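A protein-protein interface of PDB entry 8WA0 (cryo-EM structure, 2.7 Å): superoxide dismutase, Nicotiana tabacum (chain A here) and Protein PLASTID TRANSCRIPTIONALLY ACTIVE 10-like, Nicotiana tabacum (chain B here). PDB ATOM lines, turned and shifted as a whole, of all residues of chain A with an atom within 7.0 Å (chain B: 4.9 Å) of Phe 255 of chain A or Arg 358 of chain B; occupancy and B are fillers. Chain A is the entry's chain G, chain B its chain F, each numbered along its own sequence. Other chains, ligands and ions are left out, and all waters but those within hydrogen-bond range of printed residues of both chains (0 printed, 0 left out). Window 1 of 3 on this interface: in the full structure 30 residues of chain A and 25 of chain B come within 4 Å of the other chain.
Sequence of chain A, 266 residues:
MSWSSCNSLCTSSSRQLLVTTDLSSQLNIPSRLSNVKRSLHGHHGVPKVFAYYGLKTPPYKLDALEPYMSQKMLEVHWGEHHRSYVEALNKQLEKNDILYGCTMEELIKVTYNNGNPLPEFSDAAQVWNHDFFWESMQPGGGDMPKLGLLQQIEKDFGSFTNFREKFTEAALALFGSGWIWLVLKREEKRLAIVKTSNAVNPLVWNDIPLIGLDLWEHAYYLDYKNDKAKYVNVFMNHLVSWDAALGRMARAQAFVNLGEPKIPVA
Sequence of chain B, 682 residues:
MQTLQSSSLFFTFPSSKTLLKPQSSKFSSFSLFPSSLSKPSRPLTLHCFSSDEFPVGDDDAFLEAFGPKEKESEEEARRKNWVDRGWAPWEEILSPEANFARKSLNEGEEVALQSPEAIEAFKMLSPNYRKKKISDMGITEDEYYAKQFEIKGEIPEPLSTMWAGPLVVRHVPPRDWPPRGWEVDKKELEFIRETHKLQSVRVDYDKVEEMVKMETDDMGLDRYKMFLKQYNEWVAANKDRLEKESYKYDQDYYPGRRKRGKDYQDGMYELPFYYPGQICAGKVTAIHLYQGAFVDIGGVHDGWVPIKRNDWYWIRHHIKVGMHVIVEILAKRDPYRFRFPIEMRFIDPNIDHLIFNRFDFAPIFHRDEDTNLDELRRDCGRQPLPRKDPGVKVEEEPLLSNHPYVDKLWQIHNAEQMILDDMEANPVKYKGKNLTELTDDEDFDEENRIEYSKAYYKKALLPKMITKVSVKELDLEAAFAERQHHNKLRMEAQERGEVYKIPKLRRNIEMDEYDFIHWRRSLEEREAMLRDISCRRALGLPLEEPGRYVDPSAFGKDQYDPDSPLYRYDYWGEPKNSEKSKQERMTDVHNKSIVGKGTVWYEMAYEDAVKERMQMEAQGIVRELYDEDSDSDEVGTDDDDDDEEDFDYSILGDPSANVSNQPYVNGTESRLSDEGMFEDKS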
ATOM      1  N   ARG A 186     -11.698 -32.773 -10.542  1.00  0.00           N
ATOM      2  CA  ARG A 186     -12.399 -31.860  -9.685  1.00  0.00           C
ATOM      3  C   ARG A 186     -11.536 -31.080  -8.752  1.00  0.00           C
ATOM      4  O   ARG A 186     -11.706 -29.876  -8.617  1.00  0.00           O
ATOM      5  CB  ARG A 186     -13.442 -32.622  -8.897  1.00  0.00           C
ATOM      6  CG  ARG A 186     -14.620 -33.126  -9.691  1.00  0.00           C
ATOM      7  CD  ARG A 186     -15.535 -33.901  -8.773  1.00  0.00           C
ATOM      8  NE  ARG A 186     -16.879 -34.014  -9.303  1.00  0.00           N
ATOM      9  CZ  ARG A 186     -17.841 -34.724  -8.735  1.00  0.00           C
ATOM     10  NH1 ARG A 186     -17.603 -35.388  -7.616  1.00  0.00           N
ATOM     11  NH2 ARG A 186     -19.042 -34.769  -9.283  1.00  0.00           N
ATOM     12  N   ILE A 208     -14.320 -36.312 -14.260  1.00  0.00           N
ATOM     13  CA  ILE A 208     -15.449 -36.179 -15.165  1.00  0.00           C
ATOM     14  C   ILE A 208     -14.998 -36.374 -16.596  1.00  0.00           C
ATOM     15  O   ILE A 208     -14.329 -35.520 -17.160  1.00  0.00           O
ATOM     16  CB  ILE A 208     -16.119 -34.811 -15.034  1.00  0.00           C
ATOM     17  CG1 ILE A 208     -16.507 -34.549 -13.579  1.00  0.00           C
ATOM     18  CG2 ILE A 208     -17.344 -34.731 -15.930  1.00  0.00           C
ATOM     19  CD1 ILE A 208     -17.223 -33.235 -13.366  1.00  0.00           C
ATOM     20  N   ALA A 250     -20.100 -28.397 -20.532  1.00  0.00           N
ATOM     21  CA  ALA A 250     -21.104 -27.569 -19.979  1.00  0.00           C
ATOM     22  C   ALA A 250     -21.749 -28.094 -18.732  1.00  0.00           C
ATOM     23  O   ALA A 250     -21.865 -27.353 -17.756  1.00  0.00           O
ATOM     24  CB  ALA A 250     -22.150 -27.368 -21.011  1.00  0.00           C
ATOM     25  N   ARG A 251     -22.136 -29.348 -18.682  1.00  0.00           N
ATOM     26  CA  ARG A 251     -22.666 -29.888 -17.449  1.00  0.00           C
ATOM     27  C   ARG A 251     -21.585 -29.933 -16.419  1.00  0.00           C
ATOM     28  O   ARG A 251     -21.843 -29.747 -15.243  1.00  0.00           O
ATOM     29  CB  ARG A 251     -23.367 -31.213 -17.620  1.00  0.00           C
ATOM     30  CG  ARG A 251     -24.312 -31.608 -16.509  1.00  0.00           C
ATOM     31  CD  ARG A 251     -25.643 -30.904 -16.648  1.00  0.00           C
ATOM     32  NE  ARG A 251     -26.583 -31.329 -15.620  1.00  0.00           N
ATOM     33  CZ  ARG A 251     -27.812 -30.844 -15.487  1.00  0.00           C
ATOM     34  NH1 ARG A 251     -28.601 -31.291 -14.521  1.00  0.00           N
ATOM     35  NH2 ARG A 251     -28.252 -29.910 -16.321  1.00  0.00           N
ATOM     36  N   ALA A 252     -20.370 -30.191 -16.831  1.00  0.00           N
ATOM     37  CA  ALA A 252     -19.280 -30.302 -15.900  1.00  0.00           C
ATOM     38  C   ALA A 252     -19.086 -29.019 -15.160  1.00  0.00           C
ATOM     39  O   ALA A 252     -18.713 -29.036 -13.999  1.00  0.00           O
ATOM     40  CB  ALA A 252     -18.017 -30.671 -16.604  1.00  0.00           C
ATOM     41  N   GLN A 253     -19.316 -27.900 -15.813  1.00  0.00           N
ATOM     42  CA  GLN A 253     -19.135 -26.601 -15.193  1.00  0.00           C
ATOM     43  C   GLN A 253     -20.029 -26.381 -14.011  1.00  0.00           C
ATOM     44  O   GLN A 253     -19.731 -25.558 -13.169  1.00  0.00           O
ATOM     45  CB  GLN A 253     -19.148 -25.473 -16.197  1.00  0.00           C
ATOM     46  CG  GLN A 253     -17.815 -25.301 -16.890  1.00  0.00           C
ATOM     47  CD  GLN A 253     -17.780 -24.070 -17.758  1.00  0.00           C
ATOM     48  OE1 GLN A 253     -16.735 -23.701 -18.288  1.00  0.00           O
ATOM     49  NE2 GLN A 253     -18.926 -23.422 -17.906  1.00  0.00           N
ATOM     50  N   ALA A 254     -21.152 -27.047 -13.931  1.00  0.00           N
ATOM     51  CA  ALA A 254     -21.878 -26.964 -12.691  1.00  0.00           C
ATOM     52  C   ALA A 254     -21.085 -27.589 -11.565  1.00  0.00           C
ATOM     53  O   ALA A 254     -20.978 -27.000 -10.506  1.00  0.00           O
ATOM     54  CB  ALA A 254     -23.216 -27.622 -12.775  1.00  0.00           C
ATOM     55  N   PHE A 255     -20.525 -28.762 -11.756  1.00  0.00           N
ATOM     56  CA  PHE A 255     -19.680 -29.381 -10.751  1.00  0.00           C
ATOM     57  C   PHE A 255     -18.280 -28.833 -10.475  1.00  0.00           C
ATOM     58  O   PHE A 255     -17.883 -28.784  -9.324  1.00  0.00           O
ATOM     59  CB  PHE A 255     -19.775 -30.874 -10.843  1.00  0.00           C
ATOM     60  CG  PHE A 255     -21.181 -31.381 -10.840  1.00  0.00           C
ATOM     61  CD1 PHE A 255     -21.835 -31.622  -9.654  1.00  0.00           C
ATOM     62  CD2 PHE A 255     -21.854 -31.602 -12.026  1.00  0.00           C
ATOM     63  CE1 PHE A 255     -23.134 -32.078  -9.649  1.00  0.00           C
ATOM     64  CE2 PHE A 255     -23.153 -32.052 -12.030  1.00  0.00           C
ATOM     65  CZ  PHE A 255     -23.794 -32.294 -10.839  1.00  0.00           C
ATOM     66  N   VAL A 256     -17.554 -28.397 -11.483  1.00  0.00           N
ATOM     67  CA  VAL A 256     -16.272 -27.774 -11.222  1.00  0.00           C
ATOM     68  C   VAL A 256     -16.270 -26.442 -11.931  1.00  0.00           C
ATOM     69  O   VAL A 256     -16.573 -26.367 -13.108  1.00  0.00           O
ATOM     70  CB  VAL A 256     -15.110 -28.684 -11.614  1.00  0.00           C
ATOM     71  N   ASN A 257     -15.959 -25.376 -11.215  1.00  0.00           N
ATOM     72  CA  ASN A 257     -16.025 -24.052 -11.803  1.00  0.00           C
ATOM     73  C   ASN A 257     -14.639 -23.574 -12.079  1.00  0.00           C
ATOM     74  O   ASN A 257     -13.805 -23.514 -11.187  1.00  0.00           O
ATOM     75  CB  ASN A 257     -16.709 -23.086 -10.843  1.00  0.00           C
ATOM     76  CG  ASN A 257     -17.028 -21.750 -11.472  1.00  0.00           C
ATOM     77  OD1 ASN A 257     -16.817 -21.534 -12.663  1.00  0.00           O
ATOM     78  ND2 ASN A 257     -17.554 -20.846 -10.667  1.00  0.00           N
ATOM     79  N   LEU A 258     -14.391 -23.215 -13.323  1.00  0.00           N
ATOM     80  CA  LEU A 258     -13.086 -22.751 -13.708  1.00  0.00           C
ATOM     81  C   LEU A 258     -13.309 -21.301 -13.996  1.00  0.00           C
ATOM     82  O   LEU A 258     -14.165 -20.956 -14.801  1.00  0.00           O
ATOM     83  CB  LEU A 258     -12.667 -23.473 -14.973  1.00  0.00           C
ATOM     84  CG  LEU A 258     -12.913 -24.981 -14.947  1.00  0.00           C
ATOM     85  CD1 LEU A 258     -13.141 -25.536 -16.339  1.00  0.00           C
ATOM     86  CD2 LEU A 258     -11.788 -25.712 -14.238  1.00  0.00           C
ATOM     87  N   LYS B 308     -21.797 -22.178   0.363  1.00  0.00           N
ATOM     88  CA  LYS B 308     -21.117 -21.915   1.625  1.00  0.00           C
ATOM     89  C   LYS B 308     -20.221 -20.696   1.770  1.00  0.00           C
ATOM     90  O   LYS B 308     -19.495 -20.363   0.852  1.00  0.00           O
ATOM     91  CB  LYS B 308     -20.306 -23.161   1.954  1.00  0.00           C
ATOM     92  CG  LYS B 308     -19.611 -23.183   3.292  1.00  0.00           C
ATOM     93  CD  LYS B 308     -18.942 -24.526   3.507  1.00  0.00           C
ATOM     94  CE  LYS B 308     -18.222 -24.991   2.255  1.00  0.00           C
ATOM     95  NZ  LYS B 308     -17.620 -26.334   2.465  1.00  0.00           N
ATOM     96  N   LEU B 330     -30.040 -34.795  -6.879  1.00  0.00           N
ATOM     97  CA  LEU B 330     -28.812 -35.423  -7.236  1.00  0.00           C
ATOM     98  C   LEU B 330     -28.423 -36.474  -6.228  1.00  0.00           C
ATOM     99  O   LEU B 330     -27.421 -37.124  -6.441  1.00  0.00           O
ATOM    100  CB  LEU B 330     -27.723 -34.389  -7.371  1.00  0.00           C
ATOM    101  CG  LEU B 330     -27.933 -33.189  -8.281  1.00  0.00           C
ATOM    102  CD1 LEU B 330     -26.887 -32.146  -7.968  1.00  0.00           C
ATOM    103  CD2 LEU B 330     -27.848 -33.599  -9.735  1.00  0.00           C
ATOM    104  N   ASP B 352     -24.481 -20.955 -11.129  1.00  0.00           N
ATOM    105  CA  ASP B 352     -23.245 -21.695 -11.155  1.00  0.00           C
ATOM    106  C   ASP B 352     -21.979 -20.942 -11.325  1.00  0.00           C
ATOM    107  O   ASP B 352     -20.923 -21.443 -10.987  1.00  0.00           O
ATOM    108  CB  ASP B 352     -23.321 -22.861 -12.114  1.00  0.00           C
ATOM    109  CG  ASP B 352     -23.771 -22.455 -13.501  1.00  0.00           C
ATOM    110  OD1 ASP B 352     -24.946 -22.067 -13.658  1.00  0.00           O
ATOM    111  OD2 ASP B 352     -22.952 -22.541 -14.439  1.00  0.00           O
ATOM    112  N   ILE B 355     -20.664 -20.325  -7.515  1.00  0.00           N
ATOM    113  CA  ILE B 355     -20.328 -21.285  -6.472  1.00  0.00           C
ATOM    114  C   ILE B 355     -18.927 -21.795  -6.634  1.00  0.00           C
ATOM    115  O   ILE B 355     -18.692 -22.694  -7.416  1.00  0.00           O
ATOM    116  CB  ILE B 355     -21.300 -22.463  -6.440  1.00  0.00           C
ATOM    117  CG1 ILE B 355     -22.737 -21.962  -6.416  1.00  0.00           C
ATOM    118  CG2 ILE B 355     -21.045 -23.328  -5.221  1.00  0.00           C
ATOM    119  CD1 ILE B 355     -23.752 -23.069  -6.254  1.00  0.00           C
ATOM    120  N   PHE B 356     -17.981 -21.199  -5.925  1.00  0.00           N
ATOM    121  CA  PHE B 356     -16.602 -21.668  -5.966  1.00  0.00           C
ATOM    122  C   PHE B 356     -16.175 -22.611  -4.842  1.00  0.00           C
ATOM    123  O   PHE B 356     -15.238 -23.369  -5.021  1.00  0.00           O
ATOM    124  CB  PHE B 356     -15.634 -20.489  -5.985  1.00  0.00           C
ATOM    125  CG  PHE B 356     -15.658 -19.686  -7.247  1.00  0.00           C
ATOM    126  CD1 PHE B 356     -16.518 -18.615  -7.386  1.00  0.00           C
ATOM    127  CD2 PHE B 356     -14.793 -19.980  -8.281  1.00  0.00           C
ATOM    128  CE1 PHE B 356     -16.531 -17.866  -8.541  1.00  0.00           C
ATOM    129  CE2 PHE B 356     -14.799 -19.236  -9.440  1.00  0.00           C
ATOM    130  CZ  PHE B 356     -15.670 -18.176  -9.571  1.00  0.00           C
ATOM    131  N   ASN B 357     -16.829 -22.577  -3.689  1.00  0.00           N
ATOM    132  CA  ASN B 357     -16.393 -23.396  -2.557  1.00  0.00           C
ATOM    133  C   ASN B 357     -17.329 -24.564  -2.399  1.00  0.00           C
ATOM    134  O   ASN B 357     -18.537 -24.369  -2.372  1.00  0.00           O
ATOM    135  CB  ASN B 357     -16.413 -22.582  -1.276  1.00  0.00           C
ATOM    136  CG  ASN B 357     -15.576 -21.327  -1.361  1.00  0.00           C
ATOM    137  OD1 ASN B 357     -14.675 -21.223  -2.189  1.00  0.00           O
ATOM    138  ND2 ASN B 357     -15.863 -20.369  -0.492  1.00  0.00           N
ATOM    139  N   ARG B 358     -16.806 -25.782  -2.276  1.00  0.00           N
ATOM    140  CA  ARG B 358     -17.706 -26.930  -2.251  1.00  0.00           C
ATOM    141  C   ARG B 358     -17.461 -27.931  -1.156  1.00  0.00           C
ATOM    142  O   ARG B 358     -16.409 -27.933  -0.536  1.00  0.00           O
ATOM    143  CB  ARG B 358     -17.655 -27.639  -3.598  1.00  0.00           C
ATOM    144  CG  ARG B 358     -17.993 -26.740  -4.773  1.00  0.00           C
ATOM    145  CD  ARG B 358     -17.830 -27.440  -6.106  1.00  0.00           C
ATOM    146  NE  ARG B 358     -17.946 -26.497  -7.210  1.00  0.00           N
ATOM    147  CZ  ARG B 358     -19.090 -26.184  -7.807  1.00  0.00           C
ATOM    148  NH1 ARG B 358     -20.223 -26.747  -7.415  1.00  0.00           N
ATOM    149  NH2 ARG B 358     -19.097 -25.313  -8.805  1.00  0.00           N
ATOM    150  N   PHE B 359     -18.436 -28.793  -0.921  1.00  0.00           N
ATOM    151  CA  PHE B 359     -18.317 -29.777   0.137  1.00  0.00           C
ATOM    152  C   PHE B 359     -17.730 -31.021  -0.459  1.00  0.00           C
ATOM    153  O   PHE B 359     -18.199 -31.500  -1.480  1.00  0.00           O
ATOM    154  CB  PHE B 359     -19.689 -30.132   0.705  1.00  0.00           C
ATOM    155  CG  PHE B 359     -20.213 -29.165   1.720  1.00  0.00           C
ATOM    156  CD1 PHE B 359     -19.826 -29.257   3.038  1.00  0.00           C
ATOM    157  CD2 PHE B 359     -21.126 -28.196   1.362  1.00  0.00           C
ATOM    158  CE1 PHE B 359     -20.318 -28.381   3.981  1.00  0.00           C
ATOM    159  CE2 PHE B 359     -21.624 -27.316   2.297  1.00  0.00           C
ATOM    160  CZ  PHE B 359     -21.220 -27.411   3.609  1.00  0.00           C
ATOM    161  N   ASP B 360     -16.708 -31.561   0.176  1.00  0.00           N
ATOM    162  CA  ASP B 360     -16.105 -32.786  -0.304  1.00  0.00           C
ATOM    163  C   ASP B 360     -16.946 -34.009  -0.011  1.00  0.00           C
ATOM    164  O   ASP B 360     -17.285 -34.754  -0.924  1.00  0.00           O
ATOM    165  CB  ASP B 360     -14.691 -32.950   0.251  1.00  0.00           C
ATOM    166  CG  ASP B 360     -14.605 -32.772   1.762  1.00  0.00           C
ATOM    167  OD1 ASP B 360     -15.577 -32.318   2.398  1.00  0.00           O
ATOM    168  OD2 ASP B 360     -13.539 -33.094   2.322  1.00  0.00           O
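The guanidinium group (NE) of Arg 358 of chain B lies within hydrogen-bond range of the backbone carbonyl oxygen (O) of Phe 255 of chain A. O of Ala 254 of chain A sits at hydrogen-bond distance from NH2 of Arg 358 of chain B (3.0 Å). The backbone carbonyl oxygen of Asp 352 of chain B lies within hydrogen-bond range of the side-chain amide nitrogen of Asn 257 of chain A (3.4 Å).
Among the printed residues, pairs that only touch across the chains: Asn 257 of chain A with Phe 356 of chain B (3.4 Å), Asn 257 of chain A with Arg 358 of chain B (3.8 Å) and Asn 257 of chain A with Ile 355 of chain B (3.9 Å).
Of the 9 printed residues of chain B, 4 touch a printed residue of chain A.
Of the printed residues of chain B, Phe 255 of chain A touches Arg 358. Of chain A, only Ala 254 (3.0 Å), Phe 255 (3.1 Å) and Asn 257 (3.8 Å) come within 4 Å of Arg 358 of chain B. Printed residues of chain A within 4 Å of Ile 355 of chain B: Asn 257. Of the printed residues of chain B, Ala 254 of chain A touches Arg 358. Printed residues of chain A within 4 Å of Asp 352 of chain B: Asn 257. Of the printed residues of chain B, Asn 257 of chain A touches Asp 352 (3.4 Å), Ile 355 (3.9 Å), Phe 356 (3.4 Å) and Arg 358 (3.8 Å). Printed residues of chain A within 4 Å of Phe 356 of chain B: Asn 257. The nearest residue of chain B that does not touch Phe 255 of chain A is Leu 330 of chain B (4.1 Å).
The backbone carbonyl oxygen (O) of Ile 355 of chain B lies within hydrogen-bond range of the guanidinium group (NH2) of Arg 358 of chain B, at 3.0 Å.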
